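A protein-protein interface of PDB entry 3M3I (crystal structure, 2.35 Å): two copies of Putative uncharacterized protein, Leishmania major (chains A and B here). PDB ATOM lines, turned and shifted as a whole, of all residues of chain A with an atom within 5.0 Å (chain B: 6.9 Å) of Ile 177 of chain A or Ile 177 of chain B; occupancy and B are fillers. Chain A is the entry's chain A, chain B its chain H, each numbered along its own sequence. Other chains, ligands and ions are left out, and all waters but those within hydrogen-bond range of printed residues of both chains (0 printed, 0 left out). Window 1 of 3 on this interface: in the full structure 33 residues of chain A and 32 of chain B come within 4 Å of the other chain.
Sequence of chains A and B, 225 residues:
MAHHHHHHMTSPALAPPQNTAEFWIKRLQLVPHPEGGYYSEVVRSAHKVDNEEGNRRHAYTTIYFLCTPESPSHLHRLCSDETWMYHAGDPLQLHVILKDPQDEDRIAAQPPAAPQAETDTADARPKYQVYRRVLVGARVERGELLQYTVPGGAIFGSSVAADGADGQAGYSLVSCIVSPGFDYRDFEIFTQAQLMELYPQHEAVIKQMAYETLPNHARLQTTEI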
ATOM      1  N   TYR A  60     -16.637 -15.085  17.593  1.00  0.00           N
ATOM      2  CA  TYR A  60     -15.229 -15.035  17.231  1.00  0.00           C
ATOM      3  C   TYR A  60     -15.084 -14.767  15.739  1.00  0.00           C
ATOM      4  O   TYR A  60     -16.016 -14.958  14.969  1.00  0.00           O
ATOM      5  CB  TYR A  60     -14.535 -16.347  17.574  1.00  0.00           C
ATOM      6  CG  TYR A  60     -14.996 -17.503  16.717  1.00  0.00           C
ATOM      7  CD1 TYR A  60     -14.313 -17.862  15.572  1.00  0.00           C
ATOM      8  CD2 TYR A  60     -16.127 -18.224  17.044  1.00  0.00           C
ATOM      9  CE1 TYR A  60     -14.748 -18.900  14.783  1.00  0.00           C
ATOM     10  CE2 TYR A  60     -16.567 -19.275  16.250  1.00  0.00           C
ATOM     11  CZ  TYR A  60     -15.872 -19.603  15.119  1.00  0.00           C
ATOM     12  OH  TYR A  60     -16.303 -20.643  14.332  1.00  0.00           O
ATOM     13  N   THR A  61     -13.897 -14.317  15.364  1.00  0.00           N
ATOM     14  CA  THR A  61     -13.469 -14.180  13.991  1.00  0.00           C
ATOM     15  C   THR A  61     -12.047 -14.696  13.988  1.00  0.00           C
ATOM     16  O   THR A  61     -11.350 -14.549  14.980  1.00  0.00           O
ATOM     17  CB  THR A  61     -13.512 -12.710  13.517  1.00  0.00           C
ATOM     18  OG1 THR A  61     -12.727 -11.896  14.383  1.00  0.00           O
ATOM     19  CG2 THR A  61     -14.943 -12.164  13.502  1.00  0.00           C
ATOM     20  N   THR A  62     -11.623 -15.338  12.900  1.00  0.00           N
ATOM     21  CA  THR A  62     -10.247 -15.868  12.809  1.00  0.00           C
ATOM     22  C   THR A  62      -9.577 -15.406  11.530  1.00  0.00           C
ATOM     23  O   THR A  62     -10.251 -15.020  10.570  1.00  0.00           O
ATOM     24  CB  THR A  62     -10.162 -17.429  12.846  1.00  0.00           C
ATOM     25  OG1 THR A  62     -10.309 -17.945  11.520  1.00  0.00           O
ATOM     26  CG2 THR A  62     -11.221 -18.048  13.759  1.00  0.00           C
ATOM     27  N   ASP A  81      -9.833  -9.703  23.364  1.00  0.00           N
ATOM     28  CA  ASP A  81      -8.614 -10.522  23.386  1.00  0.00           C
ATOM     29  C   ASP A  81      -8.321 -11.069  22.001  1.00  0.00           C
ATOM     30  O   ASP A  81      -9.240 -11.382  21.248  1.00  0.00           O
ATOM     31  CB  ASP A  81      -8.761 -11.746  24.299  1.00  0.00           C
ATOM     32  CG  ASP A  81      -8.976 -11.402  25.749  1.00  0.00           C
ATOM     33  OD1 ASP A  81      -9.445 -12.295  26.478  1.00  0.00           O
ATOM     34  OD2 ASP A  81      -8.678 -10.269  26.175  1.00  0.00           O
ATOM     35  N   GLU A  82      -7.044 -11.222  21.686  1.00  0.00           N
ATOM     36  CA  GLU A  82      -6.633 -11.867  20.455  1.00  0.00           C
ATOM     37  C   GLU A  82      -5.590 -12.960  20.732  1.00  0.00           C
ATOM     38  O   GLU A  82      -4.536 -12.700  21.312  1.00  0.00           O
ATOM     39  CB  GLU A  82      -6.073 -10.834  19.496  1.00  0.00           C
ATOM     40  CG  GLU A  82      -5.653 -11.436  18.171  1.00  0.00           C
ATOM     41  CD  GLU A  82      -5.145 -10.410  17.188  1.00  0.00           C
ATOM     42  OE1 GLU A  82      -4.385  -9.505  17.599  1.00  0.00           O
ATOM     43  OE2 GLU A  82      -5.505 -10.533  16.004  1.00  0.00           O
ATOM     44  N   THR A  83      -5.890 -14.175  20.289  1.00  0.00           N
ATOM     45  CA  THR A  83      -5.052 -15.332  20.576  1.00  0.00           C
ATOM     46  C   THR A  83      -4.245 -15.697  19.336  1.00  0.00           C
ATOM     47  O   THR A  83      -4.814 -15.860  18.257  1.00  0.00           O
ATOM     48  CB  THR A  83      -5.911 -16.554  21.046  1.00  0.00           C
ATOM     49  OG1 THR A  83      -6.590 -16.234  22.271  1.00  0.00           O
ATOM     50  CG2 THR A  83      -5.047 -17.762  21.264  1.00  0.00           C
ATOM     51  N   MET A  85      -1.578 -18.300  17.431  1.00  0.00           N
ATOM     52  CA  MET A  85      -1.144 -19.705  17.366  1.00  0.00           C
ATOM     53  C   MET A  85      -0.059 -19.903  16.310  1.00  0.00           C
ATOM     54  O   MET A  85      -0.314 -19.650  15.152  1.00  0.00           O
ATOM     55  CB  MET A  85      -2.309 -20.608  16.961  1.00  0.00           C
ATOM     56  CG  MET A  85      -3.101 -21.215  18.087  1.00  0.00           C
ATOM     57  SD  MET A  85      -4.430 -20.223  18.762  1.00  0.00           S
ATOM     58  CE  MET A  85      -5.195 -19.477  17.323  1.00  0.00           C
ATOM     59  N   SER A 175      -1.963 -18.191  13.081  1.00  0.00           N
ATOM     60  CA  SER A 175      -3.377 -17.896  13.045  1.00  0.00           C
ATOM     61  C   SER A 175      -3.681 -16.999  14.227  1.00  0.00           C
ATOM     62  O   SER A 175      -3.080 -17.154  15.282  1.00  0.00           O
ATOM     63  CB  SER A 175      -4.204 -19.173  13.125  1.00  0.00           C
ATOM     64  OG  SER A 175      -4.082 -19.923  11.944  1.00  0.00           O
ATOM     65  N   CYS A 176      -4.595 -16.047  14.027  1.00  0.00           N
ATOM     66  CA  CYS A 176      -5.102 -15.214  15.099  1.00  0.00           C
ATOM     67  C   CYS A 176      -6.610 -15.397  15.246  1.00  0.00           C
ATOM     68  O   CYS A 176      -7.333 -15.480  14.257  1.00  0.00           O
ATOM     69  CB  CYS A 176      -4.793 -13.750  14.827  1.00  0.00           C
ATOM     70  SG  CYS A 176      -3.065 -13.390  14.554  1.00  0.00           S
ATOM     71  N   ILE A 177      -7.085 -15.444  16.486  1.00  0.00           N
ATOM     72  CA  ILE A 177      -8.528 -15.489  16.757  1.00  0.00           C
ATOM     73  C   ILE A 177      -8.875 -14.337  17.678  1.00  0.00           C
ATOM     74  O   ILE A 177      -8.303 -14.233  18.740  1.00  0.00           O
ATOM     75  CB  ILE A 177      -8.923 -16.827  17.415  1.00  0.00           C
ATOM     76  CG1 ILE A 177      -8.422 -17.995  16.574  1.00  0.00           C
ATOM     77  CG2 ILE A 177     -10.422 -16.949  17.584  1.00  0.00           C
ATOM     78  CD1 ILE A 177      -8.595 -19.310  17.279  1.00  0.00           C
ATOM     79  N   VAL A 178      -9.775 -13.453  17.255  1.00  0.00           N
ATOM     80  CA  VAL A 178     -10.272 -12.396  18.129  1.00  0.00           C
ATOM     81  C   VAL A 178     -11.655 -12.792  18.621  1.00  0.00           C
ATOM     82  O   VAL A 178     -12.491 -13.194  17.826  1.00  0.00           O
ATOM     83  CB  VAL A 178     -10.319 -11.027  17.420  1.00  0.00           C
ATOM     84  CG1 VAL A 178     -10.591  -9.922  18.434  1.00  0.00           C
ATOM     85  CG2 VAL A 178      -9.023 -10.761  16.677  1.00  0.00           C
ATOM     86  N   SER A 179     -11.865 -12.734  19.936  1.00  0.00           N
ATOM     87  CA  SER A 179     -13.153 -13.099  20.554  1.00  0.00           C
ATOM     88  C   SER A 179     -13.428 -12.332  21.848  1.00  0.00           C
ATOM     89  O   SER A 179     -12.631 -12.404  22.795  1.00  0.00           O
ATOM     90  CB  SER A 179     -13.224 -14.589  20.860  1.00  0.00           C
ATOM     91  OG  SER A 179     -14.380 -14.890  21.628  1.00  0.00           O
ATOM     92  N   ALA B  59     -16.365 -15.901  26.724  1.00  0.00           N
ATOM     93  CA  ALA B  59     -16.240 -15.547  25.294  1.00  0.00           C
ATOM     94  C   ALA B  59     -15.575 -16.657  24.481  1.00  0.00           C
ATOM     95  O   ALA B  59     -16.026 -16.971  23.381  1.00  0.00           O
ATOM     96  CB  ALA B  59     -15.463 -14.218  25.118  1.00  0.00           C
ATOM     97  N   TYR B  60     -14.511 -17.232  25.038  1.00  0.00           N
ATOM     98  CA  TYR B  60     -13.780 -18.338  24.422  1.00  0.00           C
ATOM     99  C   TYR B  60     -13.026 -19.083  25.526  1.00  0.00           C
ATOM    100  O   TYR B  60     -12.735 -18.504  26.553  1.00  0.00           O
ATOM    101  CB  TYR B  60     -12.785 -17.821  23.328  1.00  0.00           C
ATOM    102  CG  TYR B  60     -11.640 -17.013  23.907  1.00  0.00           C
ATOM    103  CD1 TYR B  60     -10.453 -17.621  24.262  1.00  0.00           C
ATOM    104  CD2 TYR B  60     -11.772 -15.653  24.155  1.00  0.00           C
ATOM    105  CE1 TYR B  60      -9.413 -16.893  24.826  1.00  0.00           C
ATOM    106  CE2 TYR B  60     -10.741 -14.916  24.733  1.00  0.00           C
ATOM    107  CZ  TYR B  60      -9.567 -15.548  25.069  1.00  0.00           C
ATOM    108  OH  TYR B  60      -8.537 -14.846  25.641  1.00  0.00           O
ATOM    109  N   THR B  61     -12.730 -20.361  25.311  1.00  0.00           N
ATOM    110  CA  THR B  61     -11.730 -21.097  26.101  1.00  0.00           C
ATOM    111  C   THR B  61     -10.725 -21.735  25.153  1.00  0.00           C
ATOM    112  O   THR B  61     -11.074 -22.039  24.022  1.00  0.00           O
ATOM    113  CB  THR B  61     -12.377 -22.211  26.924  1.00  0.00           C
ATOM    114  OG1 THR B  61     -13.077 -23.111  26.048  1.00  0.00           O
ATOM    115  CG2 THR B  61     -13.346 -21.624  27.938  1.00  0.00           C
ATOM    116  N   THR B  62      -9.479 -21.924  25.599  1.00  0.00           N
ATOM    117  CA  THR B  62      -8.439 -22.547  24.760  1.00  0.00           C
ATOM    118  C   THR B  62      -7.701 -23.669  25.483  1.00  0.00           C
ATOM    119  O   THR B  62      -7.543 -23.635  26.712  1.00  0.00           O
ATOM    120  CB  THR B  62      -7.376 -21.544  24.248  1.00  0.00           C
ATOM    121  OG1 THR B  62      -6.380 -21.326  25.254  1.00  0.00           O
ATOM    122  CG2 THR B  62      -8.002 -20.233  23.830  1.00  0.00           C
ATOM    123  N   ILE B  63      -7.269 -24.664  24.708  1.00  0.00           N
ATOM    124  CA  ILE B  63      -6.433 -25.752  25.207  1.00  0.00           C
ATOM    125  C   ILE B  63      -5.309 -26.115  24.237  1.00  0.00           C
ATOM    126  O   ILE B  63      -5.357 -25.790  23.036  1.00  0.00           O
ATOM    127  CB  ILE B  63      -7.260 -27.050  25.501  1.00  0.00           C
ATOM    128  CG1 ILE B  63      -7.792 -27.679  24.206  1.00  0.00           C
ATOM    129  CG2 ILE B  63      -8.401 -26.750  26.472  1.00  0.00           C
ATOM    130  CD1 ILE B  63      -8.505 -29.020  24.385  1.00  0.00           C
ATOM    131  N   LEU B  78     -20.456 -30.516  20.619  1.00  0.00           N
ATOM    132  CA  LEU B  78     -20.586 -29.275  21.371  1.00  0.00           C
ATOM    133  C   LEU B  78     -21.860 -28.578  20.907  1.00  0.00           C
ATOM    134  O   LEU B  78     -22.594 -29.134  20.078  1.00  0.00           O
ATOM    135  CB  LEU B  78     -19.367 -28.381  21.128  1.00  0.00           C
ATOM    136  CG  LEU B  78     -18.055 -28.972  21.651  1.00  0.00           C
ATOM    137  CD1 LEU B  78     -16.845 -28.072  21.335  1.00  0.00           C
ATOM    138  CD2 LEU B  78     -18.157 -29.234  23.145  1.00  0.00           C
ATOM    139  N   ASP B  81     -18.963 -23.506  18.087  1.00  0.00           N
ATOM    140  CA  ASP B  81     -17.912 -23.850  17.155  1.00  0.00           C
ATOM    141  C   ASP B  81     -16.620 -24.119  17.930  1.00  0.00           C
ATOM    142  O   ASP B  81     -16.347 -23.439  18.926  1.00  0.00           O
ATOM    143  CB  ASP B  81     -17.675 -22.704  16.170  1.00  0.00           C
ATOM    144  CG  ASP B  81     -18.897 -22.373  15.315  1.00  0.00           C
ATOM    145  OD1 ASP B  81     -18.921 -21.248  14.762  1.00  0.00           O
ATOM    146  OD2 ASP B  81     -19.818 -23.207  15.183  1.00  0.00           O
ATOM    147  N   GLU B  82     -15.850 -25.111  17.483  1.00  0.00           N
ATOM    148  CA  GLU B  82     -14.486 -25.339  17.978  1.00  0.00           C
ATOM    149  C   GLU B  82     -13.467 -25.217  16.845  1.00  0.00           C
ATOM    150  O   GLU B  82     -13.616 -25.837  15.796  1.00  0.00           O
ATOM    151  CB  GLU B  82     -14.356 -26.715  18.632  1.00  0.00           C
ATOM    152  CG  GLU B  82     -12.951 -27.002  19.189  1.00  0.00           C
ATOM    153  CD  GLU B  82     -12.861 -28.310  19.942  1.00  0.00           C
ATOM    154  OE1 GLU B  82     -13.603 -29.260  19.602  1.00  0.00           O
ATOM    155  OE2 GLU B  82     -12.036 -28.401  20.876  1.00  0.00           O
ATOM    156  N   THR B  83     -12.420 -24.426  17.052  1.00  0.00           N
ATOM    157  CA  THR B  83     -11.405 -24.241  16.022  1.00  0.00           C
ATOM    158  C   THR B  83     -10.082 -24.942  16.371  1.00  0.00           C
ATOM    159  O   THR B  83      -9.574 -24.811  17.477  1.00  0.00           O
ATOM    160  CB  THR B  83     -11.155 -22.749  15.759  1.00  0.00           C
ATOM    161  OG1 THR B  83     -12.384 -22.091  15.399  1.00  0.00           O
ATOM    162  CG2 THR B  83     -10.164 -22.579  14.634  1.00  0.00           C
ATOM    163  N   TRP B  84      -9.521 -25.665  15.404  1.00  0.00           N
ATOM    164  CA  TRP B  84      -8.264 -26.407  15.575  1.00  0.00           C
ATOM    165  C   TRP B  84      -7.098 -25.778  14.801  1.00  0.00           C
ATOM    166  O   TRP B  84      -7.248 -25.489  13.635  1.00  0.00           O
ATOM    167  CB  TRP B  84      -8.464 -27.835  15.066  1.00  0.00           C
ATOM    168  CG  TRP B  84      -9.497 -28.551  15.798  1.00  0.00           C
ATOM    169  CD1 TRP B  84     -10.843 -28.318  15.765  1.00  0.00           C
ATOM    170  CD2 TRP B  84      -9.296 -29.628  16.697  1.00  0.00           C
ATOM    171  NE1 TRP B  84     -11.495 -29.196  16.594  1.00  0.00           N
ATOM    172  CE2 TRP B  84     -10.568 -30.015  17.179  1.00  0.00           C
ATOM    173  CE3 TRP B  84      -8.168 -30.314  17.141  1.00  0.00           C
ATOM    174  CZ2 TRP B  84     -10.736 -31.048  18.079  1.00  0.00           C
ATOM    175  CZ3 TRP B  84      -8.339 -31.340  18.029  1.00  0.00           C
ATOM    176  CH2 TRP B  84      -9.616 -31.696  18.500  1.00  0.00           C
ATOM    177  N   MET B  85      -5.949 -25.604  15.453  1.00  0.00           N
ATOM    178  CA  MET B  85      -4.764 -24.976  14.862  1.00  0.00           C
ATOM    179  C   MET B  85      -3.581 -25.917  14.956  1.00  0.00           C
ATOM    180  O   MET B  85      -3.264 -26.357  16.051  1.00  0.00           O
ATOM    181  CB  MET B  85      -4.400 -23.692  15.623  1.00  0.00           C
ATOM    182  CG  MET B  85      -4.799 -22.364  14.948  1.00  0.00           C
ATOM    183  SD  MET B  85      -6.503 -21.788  15.170  1.00  0.00           S
ATOM    184  CE  MET B  85      -6.834 -22.246  16.875  1.00  0.00           C
ATOM    185  N   GLN B 147      -5.597 -24.560   9.882  1.00  0.00           N
ATOM    186  CA  GLN B 147      -6.683 -24.214  10.768  1.00  0.00           C
ATOM    187  C   GLN B 147      -7.970 -24.755  10.165  1.00  0.00           C
ATOM    188  O   GLN B 147      -8.081 -24.856   8.953  1.00  0.00           O
ATOM    189  CB  GLN B 147      -6.747 -22.689  10.898  1.00  0.00           C
ATOM    190  CG  GLN B 147      -7.893 -22.150  11.745  1.00  0.00           C
ATOM    191  CD  GLN B 147      -8.287 -20.736  11.355  1.00  0.00           C
ATOM    192  OE1 GLN B 147      -9.469 -20.400  11.357  1.00  0.00           O
ATOM    193  NE2 GLN B 147      -7.298 -19.906  11.009  1.00  0.00           N
ATOM    194  N   THR B 149     -12.453 -25.362  11.562  1.00  0.00           N
ATOM    195  CA  THR B 149     -13.454 -25.103  12.570  1.00  0.00           C
ATOM    196  C   THR B 149     -14.587 -26.082  12.433  1.00  0.00           C
ATOM    197  O   THR B 149     -15.275 -26.118  11.407  1.00  0.00           O
ATOM    198  CB  THR B 149     -14.070 -23.707  12.430  1.00  0.00           C
ATOM    199  OG1 THR B 149     -13.079 -22.715  12.710  1.00  0.00           O
ATOM    200  CG2 THR B 149     -15.236 -23.547  13.405  1.00  0.00           C
ATOM    201  N   SER B 175      -3.622 -26.588  19.078  1.00  0.00           N
ATOM    202  CA  SER B 175      -4.414 -25.826  20.036  1.00  0.00           C
ATOM    203  C   SER B 175      -5.879 -25.888  19.627  1.00  0.00           C
ATOM    204  O   SER B 175      -6.178 -25.821  18.438  1.00  0.00           O
ATOM    205  CB  SER B 175      -3.993 -24.358  20.054  1.00  0.00           C
ATOM    206  OG  SER B 175      -2.762 -24.177  20.706  1.00  0.00           O
ATOM    207  N   CYS B 176      -6.793 -25.989  20.594  1.00  0.00           N
ATOM    208  CA  CYS B 176      -8.210 -25.865  20.300  1.00  0.00           C
ATOM    209  C   CYS B 176      -8.811 -24.657  21.005  1.00  0.00           C
ATOM    210  O   CYS B 176      -8.441 -24.329  22.118  1.00  0.00           O
ATOM    211  CB  CYS B 176      -8.958 -27.127  20.692  1.00  0.00           C
ATOM    212  SG  CYS B 176      -8.124 -28.613  20.149  1.00  0.00           S
ATOM    213  N   ILE B 177      -9.745 -23.997  20.333  1.00  0.00           N
ATOM    214  CA  ILE B 177     -10.449 -22.860  20.882  1.00  0.00           C
ATOM    215  C   ILE B 177     -11.930 -23.076  20.657  1.00  0.00           C
ATOM    216  O   ILE B 177     -12.348 -23.264  19.526  1.00  0.00           O
ATOM    217  CB  ILE B 177      -9.986 -21.558  20.202  1.00  0.00           C
ATOM    218  CG1 ILE B 177      -8.452 -21.478  20.282  1.00  0.00           C
ATOM    219  CG2 ILE B 177     -10.678 -20.339  20.826  1.00  0.00           C
ATOM    220  CD1 ILE B 177      -7.834 -20.162  19.837  1.00  0.00           C
ATOM    221  N   VAL B 178     -12.700 -23.092  21.746  1.00  0.00           N
ATOM    222  CA  VAL B 178     -14.161 -23.170  21.706  1.00  0.00           C
ATOM    223  C   VAL B 178     -14.741 -21.784  21.995  1.00  0.00           C
ATOM    224  O   VAL B 178     -14.414 -21.191  23.021  1.00  0.00           O
ATOM    225  CB  VAL B 178     -14.720 -24.138  22.783  1.00  0.00           C
ATOM    226  CG1 VAL B 178     -16.218 -23.975  22.889  1.00  0.00           C
ATOM    227  CG2 VAL B 178     -14.361 -25.580  22.487  1.00  0.00           C
ATOM    228  N   SER B 179     -15.604 -21.284  21.108  1.00  0.00           N
ATOM    229  CA  SER B 179     -16.162 -19.945  21.228  1.00  0.00           C
ATOM    230  C   SER B 179     -17.584 -19.846  20.642  1.00  0.00           C
ATOM    231  O   SER B 179     -17.765 -20.092  19.457  1.00  0.00           O
ATOM    232  CB  SER B 179     -15.242 -18.968  20.512  1.00  0.00           C
ATOM    233  OG  SER B 179     -15.714 -17.647  20.601  1.00  0.00           O
ATOM    234  N   PRO B 180     -18.606 -19.495  21.467  1.00  0.00           N
ATOM    235  CA  PRO B 180     -18.594 -19.259  22.901  1.00  0.00           C
ATOM    236  C   PRO B 180     -18.029 -20.429  23.706  1.00  0.00           C
ATOM    237  O   PRO B 180     -17.940 -21.562  23.201  1.00  0.00           O
ATOM    238  CB  PRO B 180     -20.071 -19.025  23.231  1.00  0.00           C
ATOM    239  CG  PRO B 180     -20.624 -18.464  21.984  1.00  0.00           C
ATOM    240  CD  PRO B 180     -19.939 -19.211  20.900  1.00  0.00           C
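N of Ser 179 of chain A is in hydrogen-bond range of O of Asp 81 of chain A, 3.2 Å away. The backbone NH (N) of Met 85 of chain A lies within hydrogen-bond range of the backbone carbonyl oxygen (O) of Ser 175 of chain A, 2.9 Å away. N of Ser 179 of chain B is in hydrogen-bond range of O of Asp 81 of chain B, 3.2 Å away. The side-chain hydroxyl (OG1) of Thr 83 of chain B is in hydrogen-bond range of the side-chain hydroxyl (OG1) of Thr 149 of chain B, at 2.8 Å. The backbone carbonyl oxygen (O) of Ile 177 of chain B lies within hydrogen-bond range of the backbone NH (N) of Thr 83 of chain B, 2.7 Å away. The backbone NH (N) of Met 85 of chain B is in hydrogen-bond range of the backbone carbonyl oxygen (O) of Ser 175 of chain B (3.0 Å).
Thr 61 of chain A touches none of the printed residues of chain B. Of the printed residues of chain B, Ser 175 of chain A touches Met 85 (3.7 Å) and Gln 147 (3.3 Å). Val 178 of chain A touches none of the printed residues of chain B. Of the printed residues of chain B, Ser 179 of chain A touches Ala 59, Tyr 60 and Ser 179. Of the printed residues of chain A, Gln 147 of chain B touches Thr 62 and Ser 175. Of chain A, only Thr 83, Met 85 and Ile 177 come within 4 Å of Ile 177 of chain B. The nearest residue of chain B that does not touch Ile 177 of chain A is Thr 83 of chain B (4.5 Å). The nearest printed residue of chain A that does not touch Ile 177 of chain B is Ser 179 of chain A (6.3 Å). The nearest printed residue of chain B that does not touch Thr 62 of chain A is Thr 83 of chain B (4.5 Å).
Of the 12 printed residues of chain A, 8 touch a printed residue of chain B. Hydrophobic or aromatic side chains of chain A that line the printed part of chain B: Tyr 60, Met 85 and Ile 177.
Among the printed residues, pairs that only touch across the chains: Tyr 60 of chain A with Thr 149 of chain B, Tyr 60 of chain A with Ser 179 of chain B, Thr 83 of chain A with Tyr 60 of chain B, Thr 83 of chain A with Ile 177 of chain B, Met 85 of chain A with Met 85 of chain B, Met 85 of chain A with Ser 175 of chain B, Met 85 of chain A with Ile 177 of chain B, Ser 175 of chain A with Met 85 of chain B, Ile 177 of chain A with Met 85 of chain B, Ile 177 of chain A with Ile 177 of chain B and Ser 179 of chain A with Tyr 60 of chain B.
OD1 of Asp 81 of chain B lies within hydrogen-bond range of OH of Tyr 60 of chain A (2.7 Å). OE1 of Gln 147 of chain B is in hydrogen-bond range of OG1 of Thr 62 of chain A, at 2.6 Å. The side-chain hydroxyl (OH) of Tyr 60 of chain B is in hydrogen-bond range of the side-chain carboxylate (OD1) of Asp 81 of chain A. NE2 of Gln 147 of chain B lies within hydrogen-bond range of OG of Ser 175 of chain A (3.3 Å). The backbone carbonyl oxygen of Ala 59 of chain B sits at hydrogen-bond distance from the side-chain hydroxyl of Ser 179 of chain A (3.2 Å). OG of Ser 179 of chain A sits at hydrogen-bond distance from OG of Ser 179 of chain B (3.2 Å).
Tyr 60 of chain A touches Asp 81 of chain B, and with the chains exchanged Asp 81 of chain A touches Tyr 60 of chain B. Thr 83 of chain A touches Tyr 60 of chain B, but with the chains exchanged Tyr 60 of chain A does not touch Thr 83 of chain B (4.02 Å). Thr 83 of chain A touches Ile 177 of chain B, but with the chains exchanged Ile 177 of chain A does not touch Thr 83 of chain B (4.5 Å). Met 85 of chain A touches Ser 175 of chain B, and with the chains exchanged Ser 175 of chain A touches Met 85 of chain B.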
